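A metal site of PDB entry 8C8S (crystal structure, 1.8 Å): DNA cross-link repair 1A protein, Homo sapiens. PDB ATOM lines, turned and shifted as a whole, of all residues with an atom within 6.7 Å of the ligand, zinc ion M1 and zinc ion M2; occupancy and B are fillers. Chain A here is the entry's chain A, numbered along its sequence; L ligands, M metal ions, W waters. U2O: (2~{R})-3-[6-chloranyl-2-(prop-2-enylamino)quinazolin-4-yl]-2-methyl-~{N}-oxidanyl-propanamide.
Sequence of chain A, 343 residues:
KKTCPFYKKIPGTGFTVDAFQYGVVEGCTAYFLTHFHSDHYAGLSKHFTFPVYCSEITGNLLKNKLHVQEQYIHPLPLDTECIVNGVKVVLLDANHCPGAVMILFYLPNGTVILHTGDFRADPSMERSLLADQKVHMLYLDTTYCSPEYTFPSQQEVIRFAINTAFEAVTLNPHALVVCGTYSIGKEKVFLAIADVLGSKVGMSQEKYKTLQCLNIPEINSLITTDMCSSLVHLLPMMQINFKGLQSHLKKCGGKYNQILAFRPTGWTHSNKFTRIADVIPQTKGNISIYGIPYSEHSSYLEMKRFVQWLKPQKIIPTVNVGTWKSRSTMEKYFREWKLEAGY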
ATOM      1  N   HIS A  35      13.597 -17.840  -0.060  1.00  0.00           N
ATOM      2  CA  HIS A  35      14.808 -17.020  -0.160  1.00  0.00           C
ATOM      3  C   HIS A  35      15.407 -17.134  -1.545  1.00  0.00           C
ATOM      4  O   HIS A  35      15.073 -18.021  -2.326  1.00  0.00           O
ATOM      5  CB  HIS A  35      15.852 -17.397   0.887  1.00  0.00           C
ATOM      6  CG  HIS A  35      16.367 -18.795   0.764  1.00  0.00           C
ATOM      7  ND1 HIS A  35      15.583 -19.901   1.016  1.00  0.00           N
ATOM      8  CD2 HIS A  35      17.588 -19.264   0.432  1.00  0.00           C
ATOM      9  CE1 HIS A  35      16.314 -20.996   0.855  1.00  0.00           C
ATOM     10  NE2 HIS A  35      17.533 -20.626   0.492  1.00  0.00           N
ATOM     11  N   PHE A  36      16.366 -16.239  -1.825  1.00  0.00           N
ATOM     12  CA  PHE A  36      16.904 -16.100  -3.178  1.00  0.00           C
ATOM     13  C   PHE A  36      18.193 -16.926  -3.339  1.00  0.00           C
ATOM     14  O   PHE A  36      19.302 -16.412  -3.491  1.00  0.00           O
ATOM     15  CB  PHE A  36      17.131 -14.626  -3.495  1.00  0.00           C
ATOM     16  CG  PHE A  36      17.413 -14.358  -4.955  1.00  0.00           C
ATOM     17  CD1 PHE A  36      16.396 -14.410  -5.889  1.00  0.00           C
ATOM     18  CD2 PHE A  36      18.704 -14.032  -5.371  1.00  0.00           C
ATOM     19  CE1 PHE A  36      16.663 -14.154  -7.252  1.00  0.00           C
ATOM     20  CE2 PHE A  36      18.971 -13.776  -6.734  1.00  0.00           C
ATOM     21  CZ  PHE A  36      17.953 -13.836  -7.662  1.00  0.00           C
ATOM     22  N   HIS A  37      18.028 -18.245  -3.287  1.00  0.00           N
ATOM     23  CA  HIS A  37      19.087 -19.178  -3.661  1.00  0.00           C
ATOM     24  C   HIS A  37      18.595 -20.020  -4.836  1.00  0.00           C
ATOM     25  O   HIS A  37      17.416 -20.395  -4.876  1.00  0.00           O
ATOM     26  CB  HIS A  37      19.495 -20.087  -2.499  1.00  0.00           C
ATOM     27  CG  HIS A  37      20.455 -19.433  -1.537  1.00  0.00           C
ATOM     28  ND1 HIS A  37      20.633 -19.880  -0.248  1.00  0.00           N
ATOM     29  CD2 HIS A  37      21.295 -18.390  -1.689  1.00  0.00           C
ATOM     30  CE1 HIS A  37      21.531 -19.136   0.356  1.00  0.00           C
ATOM     31  NE2 HIS A  37      21.953 -18.221  -0.499  1.00  0.00           N
ATOM     32  N   SER A  38      19.495 -20.339  -5.759  1.00  0.00           N
ATOM     33  CA  SER A  38      19.085 -20.895  -7.053  1.00  0.00           C
ATOM     34  C   SER A  38      18.375 -22.227  -6.928  1.00  0.00           C
ATOM     35  O   SER A  38      17.468 -22.526  -7.720  1.00  0.00           O
ATOM     36  CB  SER A  38      20.284 -21.013  -7.992  1.00  0.00           C
ATOM     37  OG  SER A  38      21.327 -21.772  -7.406  1.00  0.00           O
ATOM     38  N   ASP A  39      18.741 -23.069  -5.959  1.00  0.00           N
ATOM     39  CA  ASP A  39      18.011 -24.324  -5.822  1.00  0.00           C
ATOM     40  C   ASP A  39      16.556 -24.128  -5.417  1.00  0.00           C
ATOM     41  O   ASP A  39      15.769 -25.083  -5.505  1.00  0.00           O
ATOM     42  CB  ASP A  39      18.720 -25.269  -4.838  1.00  0.00           C
ATOM     43  CG  ASP A  39      19.297 -24.562  -3.614  1.00  0.00           C
ATOM     44  OD1 ASP A  39      19.852 -23.446  -3.769  1.00  0.00           O
ATOM     45  OD2 ASP A  39      19.210 -25.130  -2.482  1.00  0.00           O
ATOM     46  N   HIS A  40      16.158 -22.910  -5.007  1.00  0.00           N
ATOM     47  CA  HIS A  40      14.798 -22.616  -4.594  1.00  0.00           C
ATOM     48  C   HIS A  40      14.015 -21.790  -5.591  1.00  0.00           C
ATOM     49  O   HIS A  40      12.812 -22.005  -5.763  1.00  0.00           O
ATOM     50  CB  HIS A  40      14.807 -21.915  -3.244  1.00  0.00           C
ATOM     51  CG  HIS A  40      15.436 -22.736  -2.168  1.00  0.00           C
ATOM     52  ND1 HIS A  40      14.705 -23.381  -1.195  1.00  0.00           N
ATOM     53  CD2 HIS A  40      16.730 -23.077  -1.949  1.00  0.00           C
ATOM     54  CE1 HIS A  40      15.516 -24.071  -0.416  1.00  0.00           C
ATOM     55  NE2 HIS A  40      16.747 -23.904  -0.861  1.00  0.00           N
ATOM     56  N   HIS A  96      19.218 -17.430   7.732  1.00  0.00           N
ATOM     57  CA  HIS A  96      19.917 -18.104   6.646  1.00  0.00           C
ATOM     58  C   HIS A  96      20.734 -17.053   5.887  1.00  0.00           C
ATOM     59  O   HIS A  96      21.699 -16.516   6.437  1.00  0.00           O
ATOM     60  CB  HIS A  96      18.905 -18.832   5.757  1.00  0.00           C
ATOM     61  CG  HIS A  96      19.506 -19.696   4.710  1.00  0.00           C
ATOM     62  ND1 HIS A  96      20.489 -20.619   4.972  1.00  0.00           N
ATOM     63  CD2 HIS A  96      19.223 -19.821   3.386  1.00  0.00           C
ATOM     64  CE1 HIS A  96      20.814 -21.253   3.863  1.00  0.00           C
ATOM     65  NE2 HIS A  96      20.064 -20.773   2.889  1.00  0.00           N
ATOM     66  N   CYS A  97      20.347 -16.715   4.677  1.00  0.00           N
ATOM     67  CA  CYS A  97      20.946 -15.607   3.929  1.00  0.00           C
ATOM     68  C   CYS A  97      20.054 -14.373   4.009  1.00  0.00           C
ATOM     69  O   CYS A  97      18.928 -14.439   4.501  1.00  0.00           O
ATOM     70  CB  CYS A  97      21.156 -16.033   2.486  1.00  0.00           C
ATOM     71  SG  CYS A  97      19.596 -16.332   1.668  1.00  0.00           S
ATOM     72  N   ALA A 100      15.963 -14.321   3.755  1.00  0.00           N
ATOM     73  CA  ALA A 100      15.449 -15.680   3.919  1.00  0.00           C
ATOM     74  C   ALA A 100      14.415 -15.729   5.039  1.00  0.00           C
ATOM     75  O   ALA A 100      14.625 -15.149   6.102  1.00  0.00           O
ATOM     76  CB  ALA A 100      16.610 -16.636   4.208  1.00  0.00           C
ATOM     77  N   GLY A 117      11.795 -23.139   5.296  1.00  0.00           N
ATOM     78  CA  GLY A 117      12.674 -22.868   4.172  1.00  0.00           C
ATOM     79  C   GLY A 117      14.038 -23.457   4.487  1.00  0.00           C
ATOM     80  O   GLY A 117      14.141 -24.539   5.071  1.00  0.00           O
ATOM     81  N   ASP A 118      15.097 -22.726   4.152  1.00  0.00           N
ATOM     82  CA  ASP A 118      16.411 -23.020   4.713  1.00  0.00           C
ATOM     83  C   ASP A 118      16.608 -22.149   5.957  1.00  0.00           C
ATOM     84  O   ASP A 118      16.327 -20.947   5.938  1.00  0.00           O
ATOM     85  CB  ASP A 118      17.534 -22.697   3.731  1.00  0.00           C
ATOM     86  CG  ASP A 118      17.660 -23.695   2.582  1.00  0.00           C
ATOM     87  OD1 ASP A 118      16.988 -24.744   2.555  1.00  0.00           O
ATOM     88  OD2 ASP A 118      18.475 -23.380   1.720  1.00  0.00           O
ATOM     89  N   ASP A 141      14.060 -28.002   7.234  1.00  0.00           N
ATOM     90  CA  ASP A 141      15.371 -28.007   6.567  1.00  0.00           C
ATOM     91  C   ASP A 141      16.272 -28.965   7.319  1.00  0.00           C
ATOM     92  O   ASP A 141      16.838 -28.627   8.367  1.00  0.00           O
ATOM     93  CB  ASP A 141      15.958 -26.593   6.532  1.00  0.00           C
ATOM     94  CG  ASP A 141      17.436 -26.566   6.110  1.00  0.00           C
ATOM     95  OD1 ASP A 141      17.942 -27.545   5.508  1.00  0.00           O
ATOM     96  OD2 ASP A 141      18.098 -25.535   6.382  1.00  0.00           O
ATOM     97  N   THR A 143      19.177 -30.304   6.223  1.00  0.00           N
ATOM     98  CA  THR A 143      20.440 -30.399   5.487  1.00  0.00           C
ATOM     99  C   THR A 143      21.492 -31.171   6.280  1.00  0.00           C
ATOM    100  O   THR A 143      22.172 -32.058   5.735  1.00  0.00           O
ATOM    101  CB  THR A 143      20.947 -28.989   5.152  1.00  0.00           C
ATOM    102  OG1 THR A 143      19.969 -28.328   4.334  1.00  0.00           O
ATOM    103  CG2 THR A 143      22.284 -29.015   4.378  1.00  0.00           C
ATOM    104  N   TYR A 144      21.626 -30.876   7.565  1.00  0.00           N
ATOM    105  CA  TYR A 144      22.634 -31.451   8.439  1.00  0.00           C
ATOM    106  C   TYR A 144      22.004 -32.259   9.563  1.00  0.00           C
ATOM    107  O   TYR A 144      22.429 -32.184  10.725  1.00  0.00           O
ATOM    108  CB  TYR A 144      23.539 -30.344   8.989  1.00  0.00           C
ATOM    109  CG  TYR A 144      24.412 -29.711   7.939  1.00  0.00           C
ATOM    110  CD1 TYR A 144      25.196 -30.499   7.118  1.00  0.00           C
ATOM    111  CD2 TYR A 144      24.445 -28.341   7.765  1.00  0.00           C
ATOM    112  CE1 TYR A 144      26.008 -29.940   6.139  1.00  0.00           C
ATOM    113  CE2 TYR A 144      25.255 -27.761   6.796  1.00  0.00           C
ATOM    114  CZ  TYR A 144      26.033 -28.573   5.992  1.00  0.00           C
ATOM    115  OH  TYR A 144      26.822 -28.029   5.020  1.00  0.00           O
ATOM    116  N   TYR A 182      29.580 -17.396  -4.078  1.00  0.00           N
ATOM    117  CA  TYR A 182      28.838 -18.129  -5.097  1.00  0.00           C
ATOM    118  C   TYR A 182      27.414 -17.636  -5.270  1.00  0.00           C
ATOM    119  O   TYR A 182      26.844 -17.813  -6.358  1.00  0.00           O
ATOM    120  CB  TYR A 182      28.812 -19.635  -4.762  1.00  0.00           C
ATOM    121  N   SER A 183      26.832 -17.039  -4.253  1.00  0.00           N
ATOM    122  CA  SER A 183      25.445 -16.585  -4.245  1.00  0.00           C
ATOM    123  C   SER A 183      25.306 -15.689  -3.017  1.00  0.00           C
ATOM    124  O   SER A 183      26.297 -15.367  -2.356  1.00  0.00           O
ATOM    125  CB  SER A 183      24.458 -17.759  -4.229  1.00  0.00           C
ATOM    126  OG  SER A 183      24.665 -18.597  -3.116  1.00  0.00           O
ATOM    127  N   ILE A 184      24.089 -15.261  -2.705  1.00  0.00           N
ATOM    128  CA  ILE A 184      23.950 -14.416  -1.528  1.00  0.00           C
ATOM    129  C   ILE A 184      24.109 -15.273  -0.268  1.00  0.00           C
ATOM    130  O   ILE A 184      24.040 -16.509  -0.298  1.00  0.00           O
ATOM    131  CB  ILE A 184      22.621 -13.643  -1.501  1.00  0.00           C
ATOM    132  CG1 ILE A 184      21.431 -14.596  -1.420  1.00  0.00           C
ATOM    133  CG2 ILE A 184      22.517 -12.705  -2.722  1.00  0.00           C
ATOM    134  CD1 ILE A 184      20.125 -13.872  -1.077  1.00  0.00           C
ATOM    135  N   LYS A 186      26.425 -15.221   3.725  1.00  0.00           N
ATOM    136  CA  LYS A 186      27.795 -15.257   4.224  1.00  0.00           C
ATOM    137  C   LYS A 186      28.536 -13.950   3.971  1.00  0.00           C
ATOM    138  O   LYS A 186      29.759 -13.916   3.992  1.00  0.00           O
ATOM    139  CB  LYS A 186      28.553 -16.450   3.614  1.00  0.00           C
ATOM    140  CG  LYS A 186      27.763 -17.787   3.726  1.00  0.00           C
ATOM    141  CD  LYS A 186      28.604 -19.046   3.394  1.00  0.00           C
ATOM    142  CE  LYS A 186      27.743 -20.309   3.431  1.00  0.00           C
ATOM    143  NZ  LYS A 186      28.580 -21.550   3.240  1.00  0.00           N
ATOM    144  N   GLY A 266      30.492 -25.048   3.692  1.00  0.00           N
ATOM    145  CA  GLY A 266      29.633 -25.553   4.747  1.00  0.00           C
ATOM    146  C   GLY A 266      30.410 -26.505   5.623  1.00  0.00           C
ATOM    147  O   GLY A 266      31.597 -26.297   5.900  1.00  0.00           O
ATOM    148  N   TRP A 267      29.752 -27.567   6.075  1.00  0.00           N
ATOM    149  CA  TRP A 267      30.439 -28.635   6.802  1.00  0.00           C
ATOM    150  C   TRP A 267      31.423 -29.355   5.893  1.00  0.00           C
ATOM    151  O   TRP A 267      31.153 -29.570   4.709  1.00  0.00           O
ATOM    152  CB  TRP A 267      29.417 -29.623   7.363  1.00  0.00           C
ATOM    153  CG  TRP A 267      30.030 -30.856   7.985  1.00  0.00           C
ATOM    154  CD1 TRP A 267      30.411 -31.007   9.290  1.00  0.00           C
ATOM    155  CD2 TRP A 267      30.322 -32.091   7.333  1.00  0.00           C
ATOM    156  NE1 TRP A 267      30.935 -32.261   9.481  1.00  0.00           N
ATOM    157  CE2 TRP A 267      30.885 -32.954   8.298  1.00  0.00           C
ATOM    158  CE3 TRP A 267      30.167 -32.561   6.026  1.00  0.00           C
ATOM    159  CZ2 TRP A 267      31.293 -34.258   7.997  1.00  0.00           C
ATOM    160  CZ3 TRP A 267      30.565 -33.864   5.723  1.00  0.00           C
ATOM    161  CH2 TRP A 267      31.122 -34.695   6.713  1.00  0.00           C
ATOM    162  N   GLU A 296      25.207 -21.412   7.106  1.00  0.00           N
ATOM    163  CA  GLU A 296      23.905 -20.784   7.254  1.00  0.00           C
ATOM    164  C   GLU A 296      22.799 -21.821   7.316  1.00  0.00           C
ATOM    165  O   GLU A 296      21.616 -21.502   7.101  1.00  0.00           O
ATOM    166  CB  GLU A 296      23.677 -19.758   6.130  1.00  0.00           C
ATOM    167  CG  GLU A 296      24.668 -18.573   6.300  1.00  0.00           C
ATOM    168  CD  GLU A 296      24.417 -17.367   5.378  1.00  0.00           C
ATOM    169  OE1 GLU A 296      23.896 -17.554   4.258  1.00  0.00           O
ATOM    170  OE2 GLU A 296      24.758 -16.233   5.795  1.00  0.00           O
ATOM    171  N   HIS A 297      23.161 -23.067   7.622  1.00  0.00           N
ATOM    172  CA  HIS A 297      22.225 -24.117   7.990  1.00  0.00           C
ATOM    173  C   HIS A 297      22.482 -24.582   9.415  1.00  0.00           C
ATOM    174  O   HIS A 297      23.630 -24.580   9.898  1.00  0.00           O
ATOM    175  CB  HIS A 297      22.343 -25.342   7.046  1.00  0.00           C
ATOM    176  CG  HIS A 297      21.900 -25.091   5.634  1.00  0.00           C
ATOM    177  ND1 HIS A 297      20.581 -25.162   5.246  1.00  0.00           N
ATOM    178  CD2 HIS A 297      22.613 -24.805   4.514  1.00  0.00           C
ATOM    179  CE1 HIS A 297      20.490 -24.915   3.953  1.00  0.00           C
ATOM    180  NE2 HIS A 297      21.709 -24.702   3.482  1.00  0.00           N
ATOM    181  N   VAL A 319      15.004 -31.832   2.838  1.00  0.00           N
ATOM    182  CA  VAL A 319      16.361 -32.021   2.328  1.00  0.00           C
ATOM    183  C   VAL A 319      16.795 -33.449   2.650  1.00  0.00           C
ATOM    184  O   VAL A 319      16.406 -34.022   3.669  1.00  0.00           O
ATOM    185  CB  VAL A 319      17.358 -30.995   2.950  1.00  0.00           C
ATOM    186  CG1 VAL A 319      18.765 -31.149   2.332  1.00  0.00           C
ATOM    187  CG2 VAL A 319      16.864 -29.559   2.790  1.00  0.00           C
HETATM  188  C1  U2O L   1      24.084 -21.331  -0.618  1.00  0.00           C
HETATM  189  C10 U2O L   1      22.753 -26.793  -3.414  1.00  0.00           C
HETATM  190  C11 U2O L   1      23.218 -26.744  -1.135  1.00  0.00           C
HETATM  191  C12 U2O L   1      23.751 -26.768   1.270  1.00  0.00           C
HETATM  192  C13 U2O L   1      24.904 -27.395   1.930  1.00  0.00           C
HETATM  193  C14 U2O L   1      25.526 -28.475   1.552  1.00  0.00           C
HETATM  194  C15 U2O L   1      22.010 -22.682  -0.195  1.00  0.00           C
HETATM  195  C2  U2O L   1      23.443 -22.718  -0.733  1.00  0.00           C
HETATM  196  C3  U2O L   1      23.467 -23.227  -2.189  1.00  0.00           C
HETATM  197  C4  U2O L   1      23.264 -24.715  -2.257  1.00  0.00           C
HETATM  198  C5  U2O L   1      22.924 -25.395  -3.476  1.00  0.00           C
HETATM  199  C6  U2O L   1      22.771 -24.734  -4.709  1.00  0.00           C
HETATM  200  C7  U2O L   1      22.455 -25.457  -5.824  1.00  0.00           C
HETATM  201  C8  U2O L   1      22.278 -26.853  -5.778  1.00  0.00           C
HETATM  202  C9  U2O L   1      22.422 -27.508  -4.591  1.00  0.00           C
HETATM  203  N1  U2O L   1      22.906 -27.463  -2.226  1.00  0.00           N
HETATM  204  N2  U2O L   1      23.359 -27.409   0.021  1.00  0.00           N
HETATM  205  N3  U2O L   1      23.406 -25.400  -1.111  1.00  0.00           N
HETATM  206  N4  U2O L   1      21.047 -22.869  -1.074  1.00  0.00           N
HETATM  207  O1  U2O L   1      19.717 -22.888  -0.665  1.00  0.00           O
HETATM  208  O2  U2O L   1      21.789 -22.524   1.005  1.00  0.00           O
HETATM  209 CL1  U2O L   1      22.258 -24.650  -7.351  1.00  0.00          CL
HETATM  210 ZN    ZN M   1      18.740 -24.583  -0.104  1.00  0.00          ZN
HETATM  211 ZN    ZN M   2      19.593 -21.533   0.861  1.00  0.00          ZN
HETATM  212  O   HOH W   1      20.287 -27.795   1.609  1.00  0.00           O
HETATM  213  O   HOH W   2      20.731 -25.100   0.564  1.00  0.00           O
HETATM  214  O   HOH W   3      17.807 -26.314   0.898  1.00  0.00           O
HETATM  215  O   HOH W   4      22.611 -21.161  -4.485  1.00  0.00           O
HETATM  216  O   HOH W   5      24.004 -22.125   2.561  1.00  0.00           O
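A ring nitrogen (NE2) of His 297 sits close to an oxygen (O2) of the ligand, 3.3 Å away.
The backbone NH (N) of Trp 267 is in hydrogen-bond range of the side-chain hydroxyl (OH) of Tyr 144, 3.1 Å away. The backbone carbonyl oxygen (O) of Glu 296 lies within hydrogen-bond range of a ring nitrogen (ND1) of His 96, at 2.6 Å. NE2 of His 37 lies close to SG of Cys 97 (3.7 Å). The side-chain carboxylate (OD2) of Asp 141 is in hydrogen-bond range of a ring nitrogen (ND1) of His 297 (2.8 Å). A ring nitrogen (ND1) of His 297 is in hydrogen-bond range of the side-chain hydroxyl (OG1) of Thr 143, at 3.4 Å. The side-chain hydroxyl (OG1) of Thr 143 sits at hydrogen-bond distance from the side-chain carboxylate (OD1) of Asp 141 (2.5 Å). O of Ile 184 is in hydrogen-bond range of NE2 of His 37 (2.7 Å).
Ser 38 touches the ligand (OG to CL1, 3.0 Å). CG2 of Thr 143 touches C13 of the ligand (3.9 Å). Tyr 144 touches the ligand. OG of Ser 183 touches C1 of the ligand (3.7 Å). Hydrophobic or aromatic side chains that line the ligand: His 37, His 40, His 96 and His 297. 11 residues have an atom within 4 Å of the ligand: His 35, His 37, Ser 38, Asp 39, His 40, His 96, Asp 118, Thr 143, Tyr 144, Ser 183 and His 297.
Three residues have an atom within 4 Å of zinc ion M1: Asp 39, His 40 and Asp 118. The nearest printed residue that does not touch zinc ion M1 is His 35 (4.2 Å).
The nearest printed residue that does not touch zinc ion M2 is His 40 (4.1 Å).
Zinc ion M1 is bound by O1 of the ligand, water W2, OD2 of Asp 118, water W3, NE2 of His 40 and OD2 of Asp 39. Zinc ion M1 has six donor atoms within binding distance.
Zinc ion M2 is bound by O1 of the ligand (2.0 Å), NE2 of His 96 (2.2 Å), ND1 of His 37 (2.2 Å), NE2 of His 35 (2.3 Å), OD2 of Asp 118 (2.3 Å) and O2 of the ligand (2.4 Å). Zinc ion M2 has six donor atoms within binding distance.
Water W2 lies within hydrogen-bond range of N4 of the ligand (2.8 Å) and NE2 of His 297 (3.1 Å). Water W1 bridges OG1 of Thr 143 (2.8 Å) and N2 of the ligand (3.5 Å).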
